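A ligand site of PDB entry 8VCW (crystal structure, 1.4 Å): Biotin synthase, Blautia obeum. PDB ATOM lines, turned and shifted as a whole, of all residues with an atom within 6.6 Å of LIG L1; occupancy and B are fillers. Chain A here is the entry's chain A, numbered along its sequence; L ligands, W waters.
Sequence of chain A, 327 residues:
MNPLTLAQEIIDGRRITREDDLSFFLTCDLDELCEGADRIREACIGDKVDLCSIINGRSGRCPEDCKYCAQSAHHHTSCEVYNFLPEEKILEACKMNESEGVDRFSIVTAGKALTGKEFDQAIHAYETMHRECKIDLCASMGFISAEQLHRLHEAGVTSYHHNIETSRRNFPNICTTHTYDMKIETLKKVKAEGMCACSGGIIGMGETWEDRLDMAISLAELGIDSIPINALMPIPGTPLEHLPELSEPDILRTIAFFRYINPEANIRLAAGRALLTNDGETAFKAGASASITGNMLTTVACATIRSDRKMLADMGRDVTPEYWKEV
Water W2 lies within hydrogen-bond range of NE2 of Gln 71 (3.2 Å) and S3 of LIG L1 (3.4 Å).
O of Glu 64 lies close to S2 of LIG L1 (3.8 Å). Merely in contact with LIG L1: Ser 72 (3.8 Å), Ala 110 (3.7 Å) and His 178 (3.9 Å). Within 4 Å of LIG L1: Cys 62, Glu 64, Cys 66, Tyr 68, Cys 69, Ser 72, Ala 110, Gly 111 and His 178.
An oxygen (O1) of LG2 L2 is bound to an iron atom (FE2) of LIG L1, 2.3 Å away.
The backbone carbonyl oxygen (O) of Gln 71 lies within hydrogen-bond range of the backbone NH (N) of Cys 62 (3.0 Å). The backbone carbonyl oxygen (O) of Glu 64 sits at hydrogen-bond distance from the side-chain hydroxyl (OG) of Ser 72, 2.7 Å away. A ring nitrogen (ND1) of His 75 lies within hydrogen-bond range of the backbone carbonyl oxygen (O) of Cys 69. The backbone NH (N) of Gly 111 lies close to the side-chain sulfur (SG) of Cys 62 (3.5 Å). The side-chain sulfur (SG) of Cys 62 sits close to the backbone NH (N) of Glu 64 (3.5 Å). The side-chain sulfur of Cys 66 lies close to the side-chain hydroxyl of Tyr 68 (3.7 Å). The backbone carbonyl oxygen of Cys 62 sits at hydrogen-bond distance from the backbone NH of Ala 73, at 2.8 Å. The side-chain carboxylate of Glu 165 lies within hydrogen-bond range of the side-chain hydroxyl of Tyr 68 (3.1 Å).
The side-chain sulfur (SG) of Cys 62 is bound to an iron atom (FE1) of LIG L1 (2.3 Å). O of Thr 109 sits close to N1 of LG2 L2, at 3.3 Å. The backbone carbonyl oxygen (O) of Tyr 68 is in hydrogen-bond range of a nitrogen (N4) of LG2 L2 (3.2 Å). The backbone carbonyl oxygen (O) of Gly 111 sits close to a nitrogen (N1) of LG2 L2 (3.1 Å). The side-chain sulfur (SG) of Cys 69 binds an iron atom (FE4) of LIG L1 (2.3 Å). SG of Cys 66 is bound to FE3 of LIG L1 (2.3 Å). OE2 of Glu 165 sits at hydrogen-bond distance from O4 of LG2 L2 (2.6 Å). A sulfur (S3) of LIG L1 sits close to the backbone NH of Gly 111 (3.7 Å). An oxygen (O2) of LG2 L2 is in salt-bridge range of the side-chain amino group of Lys 183 (3.9 Å). The side-chain hydroxyl of Tyr 68 lies close to a sulfur (S1) of LIG L1, at 3.3 Å.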
ATOM      1  N   CYS A  62      28.450  14.566  -6.006  1.00  0.00           N
ATOM      2  CA  CYS A  62      27.755  15.692  -5.421  1.00  0.00           C
ATOM      3  C   CYS A  62      27.956  15.722  -3.913  1.00  0.00           C
ATOM      4  O   CYS A  62      27.816  14.700  -3.248  1.00  0.00           O
ATOM      5  CB  CYS A  62      26.270  15.534  -5.714  1.00  0.00           C
ATOM      6  SG  CYS A  62      25.318  17.005  -5.097  1.00  0.00           S
ATOM      7  N   PRO A  63      28.235  16.887  -3.324  1.00  0.00           N
ATOM      8  CA  PRO A  63      28.449  16.939  -1.880  1.00  0.00           C
ATOM      9  C   PRO A  63      27.195  16.926  -1.050  1.00  0.00           C
ATOM     10  O   PRO A  63      27.276  16.805   0.177  1.00  0.00           O
ATOM     11  CB  PRO A  63      29.205  18.269  -1.705  1.00  0.00           C
ATOM     12  CG  PRO A  63      28.624  19.148  -2.809  1.00  0.00           C
ATOM     13  CD  PRO A  63      28.550  18.160  -3.973  1.00  0.00           C
ATOM     14  N   GLU A  64      26.041  17.118  -1.670  1.00  0.00           N
ATOM     15  CA  GLU A  64      24.808  17.115  -0.929  1.00  0.00           C
ATOM     16  C   GLU A  64      24.444  15.696  -0.513  1.00  0.00           C
ATOM     17  O   GLU A  64      24.877  14.744  -1.126  1.00  0.00           O
ATOM     18  CB  GLU A  64      23.687  17.709  -1.803  1.00  0.00           C
ATOM     19  CG  GLU A  64      24.015  19.137  -2.332  1.00  0.00           C
ATOM     20  CD  GLU A  64      24.353  20.097  -1.230  1.00  0.00           C
ATOM     21  OE1 GLU A  64      23.440  20.494  -0.478  1.00  0.00           O
ATOM     22  OE2 GLU A  64      25.549  20.459  -1.079  1.00  0.00           O
ATOM     23  N   ASP A  65      23.611  15.570   0.529  1.00  0.00           N
ATOM     24  CA  ASP A  65      23.325  14.279   1.146  1.00  0.00           C
ATOM     25  C   ASP A  65      21.901  13.761   0.915  1.00  0.00           C
ATOM     26  O   ASP A  65      21.386  13.006   1.744  1.00  0.00           O
ATOM     27  CB  ASP A  65      23.718  14.314   2.622  1.00  0.00           C
ATOM     28  CG  ASP A  65      22.807  15.137   3.467  1.00  0.00           C
ATOM     29  OD1 ASP A  65      21.963  15.880   2.951  1.00  0.00           O
ATOM     30  OD2 ASP A  65      22.951  15.005   4.692  1.00  0.00           O
ATOM     31  N   CYS A  66      21.300  14.097  -0.218  1.00  0.00           N
ATOM     32  CA  CYS A  66      19.935  13.624  -0.497  1.00  0.00           C
ATOM     33  C   CYS A  66      19.898  12.098  -0.436  1.00  0.00           C
ATOM     34  O   CYS A  66      20.613  11.431  -1.193  1.00  0.00           O
ATOM     35  CB  CYS A  66      19.582  14.087  -1.890  1.00  0.00           C
ATOM     36  SG  CYS A  66      19.753  15.843  -2.188  1.00  0.00           S
ATOM     37  N   LYS A  67      19.009  11.566   0.390  1.00  0.00           N
ATOM     38  CA  LYS A  67      19.054  10.157   0.724  1.00  0.00           C
ATOM     39  C   LYS A  67      18.711   9.253  -0.457  1.00  0.00           C
ATOM     40  O   LYS A  67      19.031   8.063  -0.432  1.00  0.00           O
ATOM     41  CB  LYS A  67      18.095   9.840   1.878  1.00  0.00           C
ATOM     42  CG  LYS A  67      18.674  10.268   3.194  1.00  0.00           C
ATOM     43  CD  LYS A  67      17.815   9.761   4.326  1.00  0.00           C
ATOM     44  CE  LYS A  67      18.305  10.247   5.654  1.00  0.00           C
ATOM     45  NZ  LYS A  67      17.241  10.183   6.701  1.00  0.00           N
ATOM     46  N   TYR A  68      18.011   9.762  -1.477  1.00  0.00           N
ATOM     47  CA  TYR A  68      17.566   8.954  -2.604  1.00  0.00           C
ATOM     48  C   TYR A  68      18.577   8.878  -3.731  1.00  0.00           C
ATOM     49  O   TYR A  68      18.395   8.054  -4.657  1.00  0.00           O
ATOM     50  CB  TYR A  68      16.242   9.542  -3.178  1.00  0.00           C
ATOM     51  CG  TYR A  68      16.325  11.030  -3.468  1.00  0.00           C
ATOM     52  CD1 TYR A  68      16.964  11.488  -4.610  1.00  0.00           C
ATOM     53  CD2 TYR A  68      15.850  11.996  -2.546  1.00  0.00           C
ATOM     54  CE1 TYR A  68      17.102  12.828  -4.875  1.00  0.00           C
ATOM     55  CE2 TYR A  68      16.014  13.346  -2.835  1.00  0.00           C
ATOM     56  CZ  TYR A  68      16.645  13.738  -3.969  1.00  0.00           C
ATOM     57  OH  TYR A  68      16.787  15.116  -4.219  1.00  0.00           O
ATOM     58  N   CYS A  69      19.607   9.736  -3.715  1.00  0.00           N
ATOM     59  CA  CYS A  69      20.288  10.063  -4.957  1.00  0.00           C
ATOM     60  C   CYS A  69      21.532   9.188  -5.189  1.00  0.00           C
ATOM     61  O   CYS A  69      22.466   9.171  -4.382  1.00  0.00           O
ATOM     62  CB  CYS A  69      20.703  11.521  -4.940  1.00  0.00           C
ATOM     63  SG  CYS A  69      21.401  12.026  -6.570  1.00  0.00           S
ATOM     64  N   ALA A  70      21.591   8.548  -6.356  1.00  0.00           N
ATOM     65  CA  ALA A  70      22.743   7.764  -6.749  1.00  0.00           C
ATOM     66  C   ALA A  70      24.006   8.619  -6.889  1.00  0.00           C
ATOM     67  O   ALA A  70      25.114   8.040  -6.842  1.00  0.00           O
ATOM     68  CB  ALA A  70      22.462   7.075  -8.080  1.00  0.00           C
ATOM     69  N   GLN A  71      23.868   9.938  -7.111  1.00  0.00           N
ATOM     70  CA  GLN A  71      25.028  10.749  -7.460  1.00  0.00           C
ATOM     71  C   GLN A  71      25.638  11.464  -6.266  1.00  0.00           C
ATOM     72  O   GLN A  71      26.606  12.236  -6.443  1.00  0.00           O
ATOM     73  CB  GLN A  71      24.715  11.705  -8.589  1.00  0.00           C
ATOM     74  CG  GLN A  71      24.081  11.005  -9.773  1.00  0.00           C
ATOM     75  CD  GLN A  71      24.012  11.830 -10.981  1.00  0.00           C
ATOM     76  OE1 GLN A  71      25.005  12.331 -11.494  1.00  0.00           O
ATOM     77  NE2 GLN A  71      22.807  12.040 -11.477  1.00  0.00           N
ATOM     78  N   SER A  72      25.063  11.285  -5.079  1.00  0.00           N
ATOM     79  CA  SER A  72      25.648  11.878  -3.878  1.00  0.00           C
ATOM     80  C   SER A  72      26.943  11.146  -3.532  1.00  0.00           C
ATOM     81  O   SER A  72      26.972   9.904  -3.436  1.00  0.00           O
ATOM     82  CB  SER A  72      24.680  11.675  -2.719  1.00  0.00           C
ATOM     83  OG  SER A  72      25.314  12.112  -1.507  1.00  0.00           O
ATOM     84  N   ALA A  73      28.007  11.914  -3.281  1.00  0.00           N
ATOM     85  CA  ALA A  73      29.267  11.326  -2.871  1.00  0.00           C
ATOM     86  C   ALA A  73      29.208  10.778  -1.455  1.00  0.00           C
ATOM     87  O   ALA A  73      30.173  10.147  -1.004  1.00  0.00           O
ATOM     88  CB  ALA A  73      30.379  12.387  -2.994  1.00  0.00           C
ATOM     89  N   HIS A  75      27.263   8.368  -0.775  1.00  0.00           N
ATOM     90  CA  HIS A  75      26.783   7.004  -1.022  1.00  0.00           C
ATOM     91  C   HIS A  75      27.745   6.334  -1.998  1.00  0.00           C
ATOM     92  O   HIS A  75      28.249   6.971  -2.923  1.00  0.00           O
ATOM     93  CB  HIS A  75      25.377   7.053  -1.669  1.00  0.00           C
ATOM     94  CG  HIS A  75      24.419   7.964  -0.955  1.00  0.00           C
ATOM     95  ND1 HIS A  75      23.414   8.663  -1.606  1.00  0.00           N
ATOM     96  CD2 HIS A  75      24.310   8.235   0.356  1.00  0.00           C
ATOM     97  CE1 HIS A  75      22.723   9.337  -0.691  1.00  0.00           C
ATOM     98  NE2 HIS A  75      23.262   9.112   0.500  1.00  0.00           N
ATOM     99  N   THR A 109      22.683  18.297 -14.248  1.00  0.00           N
ATOM    100  CA  THR A 109      24.006  18.172 -13.666  1.00  0.00           C
ATOM    101  C   THR A 109      23.944  17.808 -12.197  1.00  0.00           C
ATOM    102  O   THR A 109      23.185  18.399 -11.454  1.00  0.00           O
ATOM    103  CB  THR A 109      24.860  19.428 -13.884  1.00  0.00           C
ATOM    104  OG1 THR A 109      24.187  20.570 -13.310  1.00  0.00           O
ATOM    105  CG2 THR A 109      25.115  19.639 -15.385  1.00  0.00           C
ATOM    106  N   ALA A 110      24.774  16.863 -11.786  1.00  0.00           N
ATOM    107  CA  ALA A 110      24.952  16.599 -10.361  1.00  0.00           C
ATOM    108  C   ALA A 110      25.729  17.739  -9.740  1.00  0.00           C
ATOM    109  O   ALA A 110      26.498  18.436 -10.406  1.00  0.00           O
ATOM    110  CB  ALA A 110      25.768  15.316 -10.188  1.00  0.00           C
ATOM    111  N   GLY A 111      25.524  17.969  -8.443  1.00  0.00           N
ATOM    112  CA  GLY A 111      26.238  19.023  -7.746  1.00  0.00           C
ATOM    113  C   GLY A 111      25.282  20.000  -7.106  1.00  0.00           C
ATOM    114  O   GLY A 111      24.107  20.042  -7.459  1.00  0.00           O
ATOM    115  N   LYS A 112      25.800  20.788  -6.154  1.00  0.00           N
ATOM    116  CA  LYS A 112      24.946  21.756  -5.506  1.00  0.00           C
ATOM    117  C   LYS A 112      24.420  22.785  -6.492  1.00  0.00           C
ATOM    118  O   LYS A 112      23.243  23.158  -6.451  1.00  0.00           O
ATOM    119  CB  LYS A 112      25.747  22.433  -4.413  1.00  0.00           C
ATOM    120  CG  LYS A 112      24.870  23.310  -3.553  1.00  0.00           C
ATOM    121  CD  LYS A 112      25.658  23.959  -2.441  1.00  0.00           C
ATOM    122  CE  LYS A 112      24.646  24.391  -1.406  1.00  0.00           C
ATOM    123  NZ  LYS A 112      25.323  24.904  -0.181  1.00  0.00           N
ATOM    124  N   GLY A 142      20.669  22.788 -10.251  1.00  0.00           N
ATOM    125  CA  GLY A 142      20.785  23.083  -8.852  1.00  0.00           C
ATOM    126  C   GLY A 142      20.548  24.552  -8.516  1.00  0.00           C
ATOM    127  O   GLY A 142      19.775  25.256  -9.149  1.00  0.00           O
ATOM    128  N   PHE A 143      21.192  25.001  -7.438  1.00  0.00           N
ATOM    129  CA  PHE A 143      20.913  26.318  -6.839  1.00  0.00           C
ATOM    130  C   PHE A 143      21.661  27.476  -7.502  1.00  0.00           C
ATOM    131  O   PHE A 143      22.544  28.128  -6.929  1.00  0.00           O
ATOM    132  CB  PHE A 143      21.268  26.294  -5.360  1.00  0.00           C
ATOM    133  CG  PHE A 143      20.444  25.382  -4.575  1.00  0.00           C
ATOM    134  CD1 PHE A 143      19.162  25.748  -4.257  1.00  0.00           C
ATOM    135  CD2 PHE A 143      20.918  24.137  -4.137  1.00  0.00           C
ATOM    136  CE1 PHE A 143      18.359  24.901  -3.532  1.00  0.00           C
ATOM    137  CE2 PHE A 143      20.120  23.284  -3.392  1.00  0.00           C
ATOM    138  CZ  PHE A 143      18.841  23.678  -3.095  1.00  0.00           C
ATOM    139  N   GLU A 165      11.141  17.959  -4.199  1.00  0.00           N
ATOM    140  CA  GLU A 165      11.497  16.609  -3.715  1.00  0.00           C
ATOM    141  C   GLU A 165      10.449  16.008  -2.806  1.00  0.00           C
ATOM    142  O   GLU A 165       9.987  14.880  -3.022  1.00  0.00           O
ATOM    143  CB  GLU A 165      12.921  16.443  -3.158  1.00  0.00           C
ATOM    144  CG  GLU A 165      13.962  17.132  -4.016  1.00  0.00           C
ATOM    145  CD  GLU A 165      14.187  16.466  -5.362  1.00  0.00           C
ATOM    146  OE1 GLU A 165      13.425  15.554  -5.761  1.00  0.00           O
ATOM    147  OE2 GLU A 165      15.096  16.968  -6.087  1.00  0.00           O
ATOM    148  N   CYS A 175      17.232  15.432   3.284  1.00  0.00           N
ATOM    149  CA  CYS A 175      18.461  16.156   2.973  1.00  0.00           C
ATOM    150  C   CYS A 175      18.705  17.084   4.131  1.00  0.00           C
ATOM    151  O   CYS A 175      17.784  17.792   4.568  1.00  0.00           O
ATOM    152  CB  CYS A 175      18.263  16.972   1.702  1.00  0.00           C
ATOM    153  SG  CYS A 175      19.688  18.001   1.214  1.00  0.00           S
ATOM    154  N   HIS A 178      21.039  21.107   2.395  1.00  0.00           N
ATOM    155  CA  HIS A 178      20.304  22.278   1.909  1.00  0.00           C
ATOM    156  C   HIS A 178      18.855  22.109   2.342  1.00  0.00           C
ATOM    157  O   HIS A 178      18.483  21.097   2.940  1.00  0.00           O
ATOM    158  CB  HIS A 178      20.460  22.480   0.394  1.00  0.00           C
ATOM    159  CG  HIS A 178      19.952  21.345  -0.459  1.00  0.00           C
ATOM    160  ND1 HIS A 178      20.803  20.438  -1.066  1.00  0.00           N
ATOM    161  CD2 HIS A 178      18.704  20.967  -0.821  1.00  0.00           C
ATOM    162  CE1 HIS A 178      20.097  19.552  -1.757  1.00  0.00           C
ATOM    163  NE2 HIS A 178      18.820  19.859  -1.620  1.00  0.00           N
ATOM    164  N   LYS A 183      14.955  25.754  -2.071  1.00  0.00           N
ATOM    165  CA  LYS A 183      14.306  25.357  -3.316  1.00  0.00           C
ATOM    166  C   LYS A 183      13.285  26.403  -3.733  1.00  0.00           C
ATOM    167  O   LYS A 183      13.202  26.812  -4.904  1.00  0.00           O
ATOM    168  CB  LYS A 183      13.581  24.023  -3.097  1.00  0.00           C
ATOM    169  CG  LYS A 183      14.472  22.815  -2.828  1.00  0.00           C
ATOM    170  CD  LYS A 183      15.218  22.386  -4.090  1.00  0.00           C
ATOM    171  CE  LYS A 183      15.853  20.977  -3.901  1.00  0.00           C
ATOM    172  NZ  LYS A 183      16.185  20.526  -5.280  1.00  0.00           N
HETATM  173 FE1  LIG L   1      23.171  16.315  -5.401  1.00  0.00          FE
HETATM  174 FE2  LIG L   1      20.950  16.958  -6.954  1.00  0.00          FE
HETATM  175 FE3  LIG L   1      20.782  15.990  -4.250  1.00  0.00          FE
HETATM  176 FE4  LIG L   1      21.590  14.295  -6.171  1.00  0.00          FE
HETATM  177  S1  LIG L   1      19.513  15.293  -6.062  1.00  0.00           S
HETATM  178  S2  LIG L   1      22.588  14.543  -4.127  1.00  0.00           S
HETATM  179  S3  LIG L   1      22.796  15.607  -7.557  1.00  0.00           S
HETATM  180  S4  LIG L   1      21.651  17.970  -4.916  1.00  0.00           S
HETATM  181  N1  LG2 L   2      21.625  18.567  -8.577  1.00  0.00           N
HETATM  182  C1  LG2 L   2      20.487  19.296  -9.149  1.00  0.00           C
HETATM  183  C2  LG2 L   2      19.285  19.263  -8.229  1.00  0.00           C
HETATM  184  O1  LG2 L   2      19.258  18.438  -7.267  1.00  0.00           O
HETATM  185  O2  LG2 L   2      18.350  20.050  -8.458  1.00  0.00           O
HETATM  186  C3  LG2 L   2      20.173  18.732 -10.553  1.00  0.00           C
HETATM  187  C4  LG2 L   2      19.829  17.229 -10.636  1.00  0.00           C
HETATM  188  S1  LG2 L   2      18.296  16.710  -9.833  1.00  0.00           S
HETATM  189  C5  LG2 L   2      17.126  17.402 -11.008  1.00  0.00           C
HETATM  190  C6  LG2 L   2      17.866  15.020 -10.333  1.00  0.00           C
HETATM  191  C7  LG2 L   2      16.387  14.674  -9.988  1.00  0.00           C
HETATM  192  O3  LG2 L   2      16.255  13.267 -10.080  1.00  0.00           O
HETATM  193  C8  LG2 L   2      16.091  14.994  -8.550  1.00  0.00           C
HETATM  194  O4  LG2 L   2      15.500  16.307  -8.547  1.00  0.00           O
HETATM  195  C9  LG2 L   2      15.170  13.896  -8.087  1.00  0.00           C
HETATM  196  O5  LG2 L   2      13.825  14.315  -8.001  1.00  0.00           O
HETATM  197  C10 LG2 L   2      15.244  12.817  -9.197  1.00  0.00           C
HETATM  198  N2  LG2 L   2      15.820  11.544  -8.661  1.00  0.00           N
HETATM  199  C11 LG2 L   2      17.110  11.370  -8.275  1.00  0.00           C
HETATM  200  N3  LG2 L   2      17.213  10.144  -7.758  1.00  0.00           N
HETATM  201  C12 LG2 L   2      16.005   9.489  -7.862  1.00  0.00           C
HETATM  202  C13 LG2 L   2      15.557   8.245  -7.532  1.00  0.00           C
HETATM  203  N4  LG2 L   2      16.354   7.281  -6.972  1.00  0.00           N
HETATM  204  N5  LG2 L   2      14.261   7.888  -7.746  1.00  0.00           N
HETATM  205  C14 LG2 L   2      13.419   8.827  -8.281  1.00  0.00           C
HETATM  206  N6  LG2 L   2      13.818  10.068  -8.621  1.00  0.00           N
HETATM  207  C15 LG2 L   2      15.116  10.406  -8.414  1.00  0.00           C
HETATM  208  O   HOH W   1      21.248  20.990  -6.023  1.00  0.00           O
HETATM  209  O   HOH W   2      21.531  14.811 -10.632  1.00  0.00           O
